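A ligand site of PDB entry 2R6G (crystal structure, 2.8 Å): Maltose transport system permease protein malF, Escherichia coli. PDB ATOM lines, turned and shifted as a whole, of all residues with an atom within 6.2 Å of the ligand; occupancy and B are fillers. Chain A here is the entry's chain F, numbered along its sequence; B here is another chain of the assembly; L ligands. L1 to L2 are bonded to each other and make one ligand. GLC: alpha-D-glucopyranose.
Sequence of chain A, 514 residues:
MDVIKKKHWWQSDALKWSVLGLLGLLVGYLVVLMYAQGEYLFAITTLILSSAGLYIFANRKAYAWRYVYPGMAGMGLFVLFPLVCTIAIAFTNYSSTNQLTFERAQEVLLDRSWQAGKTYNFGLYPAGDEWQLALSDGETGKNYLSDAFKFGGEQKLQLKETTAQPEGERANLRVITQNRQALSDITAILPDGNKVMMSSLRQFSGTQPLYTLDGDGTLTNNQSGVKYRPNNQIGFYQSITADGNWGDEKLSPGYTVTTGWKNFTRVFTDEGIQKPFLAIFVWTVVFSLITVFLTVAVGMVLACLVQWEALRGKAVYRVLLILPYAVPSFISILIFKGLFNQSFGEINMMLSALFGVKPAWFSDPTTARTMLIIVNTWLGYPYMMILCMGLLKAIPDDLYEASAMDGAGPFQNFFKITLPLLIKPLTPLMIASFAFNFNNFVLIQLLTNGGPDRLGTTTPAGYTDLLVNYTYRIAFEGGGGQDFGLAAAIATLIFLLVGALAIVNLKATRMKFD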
ATOM      1  N   THR A 291       4.299  26.591  28.365  1.00  0.00           N
ATOM      2  CA  THR A 291       4.972  25.302  28.195  1.00  0.00           C
ATOM      3  C   THR A 291       6.191  25.525  27.306  1.00  0.00           C
ATOM      4  O   THR A 291       7.288  25.156  27.681  1.00  0.00           O
ATOM      5  CB  THR A 291       4.051  24.228  27.569  1.00  0.00           C
ATOM      6  OG1 THR A 291       3.028  23.882  28.503  1.00  0.00           O
ATOM      7  CG2 THR A 291       4.843  22.974  27.218  1.00  0.00           C
ATOM      8  N   THR A 295       9.833  25.039  28.754  1.00  0.00           N
ATOM      9  CA  THR A 295      10.460  23.934  28.040  1.00  0.00           C
ATOM     10  C   THR A 295      11.768  24.367  27.367  1.00  0.00           C
ATOM     11  O   THR A 295      12.789  23.694  27.486  1.00  0.00           O
ATOM     12  CB  THR A 295       9.474  23.303  27.017  1.00  0.00           C
ATOM     13  OG1 THR A 295       8.360  22.744  27.722  1.00  0.00           O
ATOM     14  CG2 THR A 295      10.125  22.222  26.196  1.00  0.00           C
ATOM     15  N   TYR A 325      12.338  11.446  28.576  1.00  0.00           N
ATOM     16  CA  TYR A 325      11.969  11.333  27.164  1.00  0.00           C
ATOM     17  C   TYR A 325      12.209   9.916  26.637  1.00  0.00           C
ATOM     18  O   TYR A 325      11.603   9.521  25.638  1.00  0.00           O
ATOM     19  CB  TYR A 325      12.760  12.362  26.351  1.00  0.00           C
ATOM     20  CG  TYR A 325      12.118  12.818  25.056  1.00  0.00           C
ATOM     21  CD1 TYR A 325      10.726  12.912  24.928  1.00  0.00           C
ATOM     22  CD2 TYR A 325      12.905  13.193  23.970  1.00  0.00           C
ATOM     23  CE1 TYR A 325      10.148  13.344  23.737  1.00  0.00           C
ATOM     24  CE2 TYR A 325      12.331  13.632  22.783  1.00  0.00           C
ATOM     25  CZ  TYR A 325      10.953  13.710  22.673  1.00  0.00           C
ATOM     26  OH  TYR A 325      10.391  14.130  21.492  1.00  0.00           O
ATOM     27  N   SER A 329       5.475   8.327  27.204  1.00  0.00           N
ATOM     28  CA  SER A 329       4.648   9.306  27.928  1.00  0.00           C
ATOM     29  C   SER A 329       3.519   8.670  28.740  1.00  0.00           C
ATOM     30  O   SER A 329       3.355   8.975  29.916  1.00  0.00           O
ATOM     31  CB  SER A 329       4.079  10.351  26.970  1.00  0.00           C
ATOM     32  OG  SER A 329       5.019  11.375  26.715  1.00  0.00           O
ATOM     33  N   ILE A 333       2.734   9.929  32.612  1.00  0.00           N
ATOM     34  CA  ILE A 333       1.580  10.768  32.918  1.00  0.00           C
ATOM     35  C   ILE A 333       0.676  10.108  33.973  1.00  0.00           C
ATOM     36  O   ILE A 333       0.166  10.776  34.875  1.00  0.00           O
ATOM     37  CB  ILE A 333       0.753  11.106  31.651  1.00  0.00           C
ATOM     38  CG1 ILE A 333       1.653  11.704  30.557  1.00  0.00           C
ATOM     39  CG2 ILE A 333      -0.386  12.075  31.975  1.00  0.00           C
ATOM     40  CD1 ILE A 333       1.028  11.706  29.162  1.00  0.00           C
ATOM     41  N   ASN A 376       4.080  18.759  31.956  1.00  0.00           N
ATOM     42  CA  ASN A 376       4.459  18.990  30.567  1.00  0.00           C
ATOM     43  C   ASN A 376       5.901  19.503  30.419  1.00  0.00           C
ATOM     44  O   ASN A 376       6.586  19.172  29.451  1.00  0.00           O
ATOM     45  CB  ASN A 376       3.484  19.957  29.896  1.00  0.00           C
ATOM     46  CG  ASN A 376       3.207  19.606  28.443  1.00  0.00           C
ATOM     47  OD1 ASN A 376       3.472  18.492  27.990  1.00  0.00           O
ATOM     48  ND2 ASN A 376       2.643  20.555  27.701  1.00  0.00           N
ATOM     49  N   THR A 377       6.338  20.303  31.394  1.00  0.00           N
ATOM     50  CA  THR A 377       7.719  20.788  31.456  1.00  0.00           C
ATOM     51  C   THR A 377       8.684  19.606  31.635  1.00  0.00           C
ATOM     52  O   THR A 377       9.686  19.504  30.932  1.00  0.00           O
ATOM     53  CB  THR A 377       7.903  21.815  32.598  1.00  0.00           C
ATOM     54  OG1 THR A 377       7.159  22.996  32.289  1.00  0.00           O
ATOM     55  CG2 THR A 377       9.365  22.195  32.788  1.00  0.00           C
ATOM     56  N   LEU A 379       7.933  16.616  30.913  1.00  0.00           N
ATOM     57  CA  LEU A 379       7.697  15.765  29.759  1.00  0.00           C
ATOM     58  C   LEU A 379       8.388  16.281  28.491  1.00  0.00           C
ATOM     59  O   LEU A 379       8.734  15.495  27.599  1.00  0.00           O
ATOM     60  CB  LEU A 379       6.189  15.646  29.532  1.00  0.00           C
ATOM     61  CG  LEU A 379       5.605  14.391  28.878  1.00  0.00           C
ATOM     62  CD1 LEU A 379       6.137  13.099  29.515  1.00  0.00           C
ATOM     63  CD2 LEU A 379       4.091  14.446  28.963  1.00  0.00           C
ATOM     64  N   GLY A 380       8.587  17.595  28.411  1.00  0.00           N
ATOM     65  CA  GLY A 380       9.023  18.227  27.182  1.00  0.00           C
ATOM     66  C   GLY A 380      10.384  18.908  27.170  1.00  0.00           C
ATOM     67  O   GLY A 380      10.897  19.234  26.101  1.00  0.00           O
ATOM     68  N   TYR A 381      10.970  19.125  28.353  1.00  0.00           N
ATOM     69  CA  TYR A 381      12.269  19.795  28.434  1.00  0.00           C
ATOM     70  C   TYR A 381      13.406  19.043  27.715  1.00  0.00           C
ATOM     71  O   TYR A 381      14.249  19.686  27.076  1.00  0.00           O
ATOM     72  CB  TYR A 381      12.649  20.178  29.880  1.00  0.00           C
ATOM     73  CG  TYR A 381      13.337  19.094  30.679  1.00  0.00           C
ATOM     74  CD1 TYR A 381      14.691  18.827  30.508  1.00  0.00           C
ATOM     75  CD2 TYR A 381      12.627  18.322  31.604  1.00  0.00           C
ATOM     76  CE1 TYR A 381      15.330  17.824  31.221  1.00  0.00           C
ATOM     77  CE2 TYR A 381      13.255  17.320  32.326  1.00  0.00           C
ATOM     78  CZ  TYR A 381      14.609  17.077  32.132  1.00  0.00           C
ATOM     79  OH  TYR A 381      15.252  16.083  32.827  1.00  0.00           O
ATOM     80  N   TYR A 383      13.313  17.386  25.067  1.00  0.00           N
ATOM     81  CA  TYR A 383      13.172  17.681  23.644  1.00  0.00           C
ATOM     82  C   TYR A 383      13.964  18.929  23.255  1.00  0.00           C
ATOM     83  O   TYR A 383      14.685  18.916  22.259  1.00  0.00           O
ATOM     84  CB  TYR A 383      11.696  17.843  23.259  1.00  0.00           C
ATOM     85  CG  TYR A 383      11.479  18.284  21.829  1.00  0.00           C
ATOM     86  CD1 TYR A 383      11.624  17.383  20.773  1.00  0.00           C
ATOM     87  CD2 TYR A 383      11.110  19.590  21.527  1.00  0.00           C
ATOM     88  CE1 TYR A 383      11.417  17.780  19.460  1.00  0.00           C
ATOM     89  CE2 TYR A 383      10.900  20.003  20.210  1.00  0.00           C
ATOM     90  CZ  TYR A 383      11.061  19.090  19.185  1.00  0.00           C
ATOM     91  OH  TYR A 383      10.861  19.479  17.881  1.00  0.00           O
ATOM     92  N   MET A 384      13.824  19.995  24.028  1.00  0.00           N
ATOM     93  CA  MET A 384      14.510  21.257  23.744  1.00  0.00           C
ATOM     94  C   MET A 384      16.011  21.192  24.022  1.00  0.00           C
ATOM     95  O   MET A 384      16.795  21.797  23.296  1.00  0.00           O
ATOM     96  CB  MET A 384      13.879  22.427  24.498  1.00  0.00           C
ATOM     97  CG  MET A 384      12.489  22.821  23.979  1.00  0.00           C
ATOM     98  SD  MET A 384      12.428  23.374  22.265  1.00  0.00           S
ATOM     99  CE  MET A 384      10.666  23.321  21.965  1.00  0.00           C
ATOM    100  N   LEU A 429      10.976  26.063  15.732  1.00  0.00           N
ATOM    101  CA  LEU A 429      10.837  24.877  16.578  1.00  0.00           C
ATOM    102  C   LEU A 429       9.916  25.087  17.774  1.00  0.00           C
ATOM    103  O   LEU A 429       9.340  24.129  18.287  1.00  0.00           O
ATOM    104  CB  LEU A 429      12.210  24.393  17.030  1.00  0.00           C
ATOM    105  CG  LEU A 429      13.005  23.714  15.919  1.00  0.00           C
ATOM    106  CD1 LEU A 429      14.494  23.979  16.051  1.00  0.00           C
ATOM    107  CD2 LEU A 429      12.705  22.220  15.872  1.00  0.00           C
ATOM    108  N   ALA A 432       6.120  25.672  16.381  1.00  0.00           N
ATOM    109  CA  ALA A 432       5.628  24.325  16.088  1.00  0.00           C
ATOM    110  C   ALA A 432       5.306  23.607  17.383  1.00  0.00           C
ATOM    111  O   ALA A 432       4.358  22.823  17.453  1.00  0.00           O
ATOM    112  CB  ALA A 432       6.656  23.545  15.286  1.00  0.00           C
ATOM    113  N   SER A 433       6.095  23.876  18.422  1.00  0.00           N
ATOM    114  CA  SER A 433       5.846  23.321  19.740  1.00  0.00           C
ATOM    115  C   SER A 433       4.613  23.954  20.372  1.00  0.00           C
ATOM    116  O   SER A 433       3.923  23.316  21.171  1.00  0.00           O
ATOM    117  CB  SER A 433       7.053  23.514  20.649  1.00  0.00           C
ATOM    118  OG  SER A 433       6.875  22.820  21.875  1.00  0.00           O
ATOM    119  N   PHE A 434       4.344  25.210  20.014  1.00  0.00           N
ATOM    120  CA  PHE A 434       3.123  25.882  20.432  1.00  0.00           C
ATOM    121  C   PHE A 434       1.895  25.173  19.856  1.00  0.00           C
ATOM    122  O   PHE A 434       0.899  24.972  20.548  1.00  0.00           O
ATOM    123  CB  PHE A 434       3.140  27.358  20.025  1.00  0.00           C
ATOM    124  CG  PHE A 434       1.847  28.083  20.316  1.00  0.00           C
ATOM    125  CD1 PHE A 434       0.908  28.284  19.320  1.00  0.00           C
ATOM    126  CD2 PHE A 434       1.581  28.557  21.600  1.00  0.00           C
ATOM    127  CE1 PHE A 434      -0.287  28.956  19.586  1.00  0.00           C
ATOM    128  CE2 PHE A 434       0.387  29.232  21.880  1.00  0.00           C
ATOM    129  CZ  PHE A 434      -0.544  29.425  20.871  1.00  0.00           C
ATOM    130  N   PHE A 436       1.811  22.011  18.715  1.00  0.00           N
ATOM    131  CA  PHE A 436       1.760  20.663  19.272  1.00  0.00           C
ATOM    132  C   PHE A 436       1.027  20.665  20.608  1.00  0.00           C
ATOM    133  O   PHE A 436       0.114  19.870  20.826  1.00  0.00           O
ATOM    134  CB  PHE A 436       3.177  20.091  19.426  1.00  0.00           C
ATOM    135  CG  PHE A 436       3.204  18.698  20.003  1.00  0.00           C
ATOM    136  CD1 PHE A 436       3.361  18.510  21.377  1.00  0.00           C
ATOM    137  CD2 PHE A 436       3.084  17.587  19.185  1.00  0.00           C
ATOM    138  CE1 PHE A 436       3.386  17.231  21.926  1.00  0.00           C
ATOM    139  CE2 PHE A 436       3.113  16.292  19.716  1.00  0.00           C
ATOM    140  CZ  PHE A 436       3.264  16.116  21.094  1.00  0.00           C
ATOM    141  N   ASN A 437       1.430  21.580  21.492  1.00  0.00           N
ATOM    142  CA  ASN A 437       0.824  21.692  22.816  1.00  0.00           C
ATOM    143  C   ASN A 437      -0.514  22.423  22.820  1.00  0.00           C
ATOM    144  O   ASN A 437      -1.213  22.460  23.843  1.00  0.00           O
ATOM    145  CB  ASN A 437       1.808  22.343  23.804  1.00  0.00           C
ATOM    146  CG  ASN A 437       2.970  21.435  24.151  1.00  0.00           C
ATOM    147  OD1 ASN A 437       2.772  20.316  24.632  1.00  0.00           O
ATOM    148  ND2 ASN A 437       4.185  21.927  23.932  1.00  0.00           N
ATOM    149  N   ASN A 440      -2.498  19.114  22.637  1.00  0.00           N
ATOM    150  CA  ASN A 440      -1.929  18.006  23.399  1.00  0.00           C
ATOM    151  C   ASN A 440      -3.021  17.231  24.123  1.00  0.00           C
ATOM    152  O   ASN A 440      -3.125  17.259  25.355  1.00  0.00           O
ATOM    153  CB  ASN A 440      -0.850  18.502  24.371  1.00  0.00           C
ATOM    154  CG  ASN A 440       0.182  17.427  24.703  1.00  0.00           C
ATOM    155  OD1 ASN A 440      -0.146  16.245  24.824  1.00  0.00           O
ATOM    156  ND2 ASN A 440       1.438  17.836  24.848  1.00  0.00           N
ATOM    157  N   LEU A 443      -2.159  14.261  27.058  1.00  0.00           N
ATOM    158  CA  LEU A 443      -1.738  14.729  28.383  1.00  0.00           C
ATOM    159  C   LEU A 443      -2.911  15.118  29.278  1.00  0.00           C
ATOM    160  O   LEU A 443      -2.895  14.851  30.483  1.00  0.00           O
ATOM    161  CB  LEU A 443      -0.758  15.896  28.258  1.00  0.00           C
ATOM    162  CG  LEU A 443      -0.266  16.543  29.557  1.00  0.00           C
ATOM    163  CD1 LEU A 443       0.759  15.666  30.268  1.00  0.00           C
ATOM    164  CD2 LEU A 443       0.307  17.919  29.288  1.00  0.00           C
ATOM    165  N   LEU B 172       9.487  19.438  10.181  1.00  0.00           N
ATOM    166  CA  LEU B 172      10.125  19.941  11.404  1.00  0.00           C
ATOM    167  C   LEU B 172      11.647  19.951  11.284  1.00  0.00           C
ATOM    168  O   LEU B 172      12.281  20.959  11.568  1.00  0.00           O
ATOM    169  CB  LEU B 172       9.667  19.113  12.630  1.00  0.00           C
ATOM    170  CG  LEU B 172      10.028  17.610  12.785  1.00  0.00           C
ATOM    171  CD1 LEU B 172      10.089  17.190  14.256  1.00  0.00           C
ATOM    172  CD2 LEU B 172       9.084  16.694  12.001  1.00  0.00           C
ATOM    173  N   LEU B 221      16.265  12.295  17.899  1.00  0.00           N
ATOM    174  CA  LEU B 221      14.871  12.737  18.006  1.00  0.00           C
ATOM    175  C   LEU B 221      13.901  11.838  17.235  1.00  0.00           C
ATOM    176  O   LEU B 221      12.834  11.494  17.734  1.00  0.00           O
ATOM    177  CB  LEU B 221      14.712  14.185  17.547  1.00  0.00           C
ATOM    178  CG  LEU B 221      15.110  15.287  18.537  1.00  0.00           C
ATOM    179  CD1 LEU B 221      15.092  16.647  17.857  1.00  0.00           C
ATOM    180  CD2 LEU B 221      14.204  15.290  19.766  1.00  0.00           C
ATOM    181  N   ILE B 224      13.852   8.165  18.840  1.00  0.00           N
ATOM    182  CA  ILE B 224      12.955   8.086  19.989  1.00  0.00           C
ATOM    183  C   ILE B 224      11.492   8.178  19.565  1.00  0.00           C
ATOM    184  O   ILE B 224      10.651   7.462  20.093  1.00  0.00           O
ATOM    185  CB  ILE B 224      13.306   9.096  21.163  1.00  0.00           C
ATOM    186  CG1 ILE B 224      12.604  10.449  20.996  1.00  0.00           C
ATOM    187  CG2 ILE B 224      14.816   9.243  21.381  1.00  0.00           C
ATOM    188  CD1 ILE B 224      11.241  10.502  21.652  1.00  0.00           C
ATOM    189  N   ALA B 225      11.206   9.051  18.605  1.00  0.00           N
ATOM    190  CA  ALA B 225       9.838   9.253  18.128  1.00  0.00           C
ATOM    191  C   ALA B 225       9.229   7.950  17.627  1.00  0.00           C
ATOM    192  O   ALA B 225       8.054   7.670  17.872  1.00  0.00           O
ATOM    193  CB  ALA B 225       9.795  10.316  17.029  1.00  0.00           C
HETATM  194  C1  GLC L   1       8.002  17.030  18.235  1.00  0.00           C
HETATM  195  C2  GLC L   1       8.342  15.706  18.948  1.00  0.00           C
HETATM  196  C3  GLC L   1       7.468  15.488  20.174  1.00  0.00           C
HETATM  197  C4  GLC L   1       7.548  16.685  21.113  1.00  0.00           C
HETATM  198  C5  GLC L   1       7.153  17.960  20.354  1.00  0.00           C
HETATM  199  C6  GLC L   1       7.329  19.197  21.231  1.00  0.00           C
HETATM  200  O1  GLC L   1       6.775  16.923  17.517  1.00  0.00           O
HETATM  201  O2  GLC L   1       8.213  14.594  18.048  1.00  0.00           O
HETATM  202  O3  GLC L   1       7.892  14.298  20.866  1.00  0.00           O
HETATM  203  O4  GLC L   1       6.693  16.478  22.237  1.00  0.00           O
HETATM  204  O5  GLC L   1       7.947  18.125  19.175  1.00  0.00           O
HETATM  205  O6  GLC L   1       6.339  20.170  20.874  1.00  0.00           O
HETATM  206  C1  GLC L   2       7.393  16.345  23.478  1.00  0.00           C
HETATM  207  C2  GLC L   2       7.003  15.032  24.175  1.00  0.00           C
HETATM  208  C3  GLC L   2       5.595  15.077  24.750  1.00  0.00           C
HETATM  209  C4  GLC L   2       5.371  16.328  25.587  1.00  0.00           C
HETATM  210  C5  GLC L   2       5.779  17.579  24.810  1.00  0.00           C
HETATM  211  C6  GLC L   2       5.667  18.834  25.663  1.00  0.00           C
HETATM  212  O2  GLC L   2       7.076  13.952  23.235  1.00  0.00           O
HETATM  213  O3  GLC L   2       5.395  13.923  25.562  1.00  0.00           O
HETATM  214  O4  GLC L   2       3.991  16.400  25.956  1.00  0.00           O
HETATM  215  O5  GLC L   2       7.127  17.453  24.342  1.00  0.00           O
HETATM  216  O6  GLC L   2       5.860  19.996  24.842  1.00  0.00           O
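The backbone carbonyl oxygen (O) of Thr 291 sits at hydrogen-bond distance from the side-chain hydroxyl (OG1) of Thr 295. OD1 of Asn 437 lies within hydrogen-bond range of ND2 of Asn 440 (2.8 Å). The side-chain amide nitrogen of Asn 376 sits close to the side-chain hydroxyl of Thr 291 (3.4 Å). OD1 of Asn 437 sits at hydrogen-bond distance from ND2 of Asn 376 (3.1 Å). ND2 of Asn 437 lies within hydrogen-bond range of O of Ser 433.
Thr 291 touches the ligand. CG of Leu 379 touches O3 of GLC L2 (3.4 Å). CA of Gly 380 touches O5 of GLC L2, 3.5 Å away. CE1 of Phe 436 touches O4 of GLC L1, 3.4 Å away. Hydrophobic or aromatic side chains within 4 Å of the ligand: Tyr 325, Leu 379, Tyr 383 and Phe 436. 11 residues have an atom within 4 Å of the ligand: Thr 291, Tyr 325, Ser 329, Asn 376, Leu 379, Gly 380, Tyr 383, Ser 433, Phe 436, Asn 437 and Asn 440. The nearest printed residue that does not touch the ligand is Leu 172 of chain B (4.5 Å).
OH of Tyr 383 sits close to O5 of GLC L1 (3.5 Å). An oxygen (O3) of GLC L1 lies within hydrogen-bond range of the side-chain hydroxyl of Tyr 325 (2.6 Å). The side-chain amide nitrogen (ND2) of Asn 440 is in hydrogen-bond range of an oxygen (O4) of GLC L2, at 3.1 Å. The side-chain amide nitrogen (ND2) of Asn 437 is in hydrogen-bond range of an oxygen (O6) of GLC L2, 2.7 Å away. OD1 of Asn 376 lies within hydrogen-bond range of O4 of GLC L2, 3.0 Å away. O6 of GLC L1 sits at hydrogen-bond distance from OG of Ser 433, at 2.9 Å. OG of Ser 329 lies within hydrogen-bond range of O3 of GLC L2 (2.8 Å).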
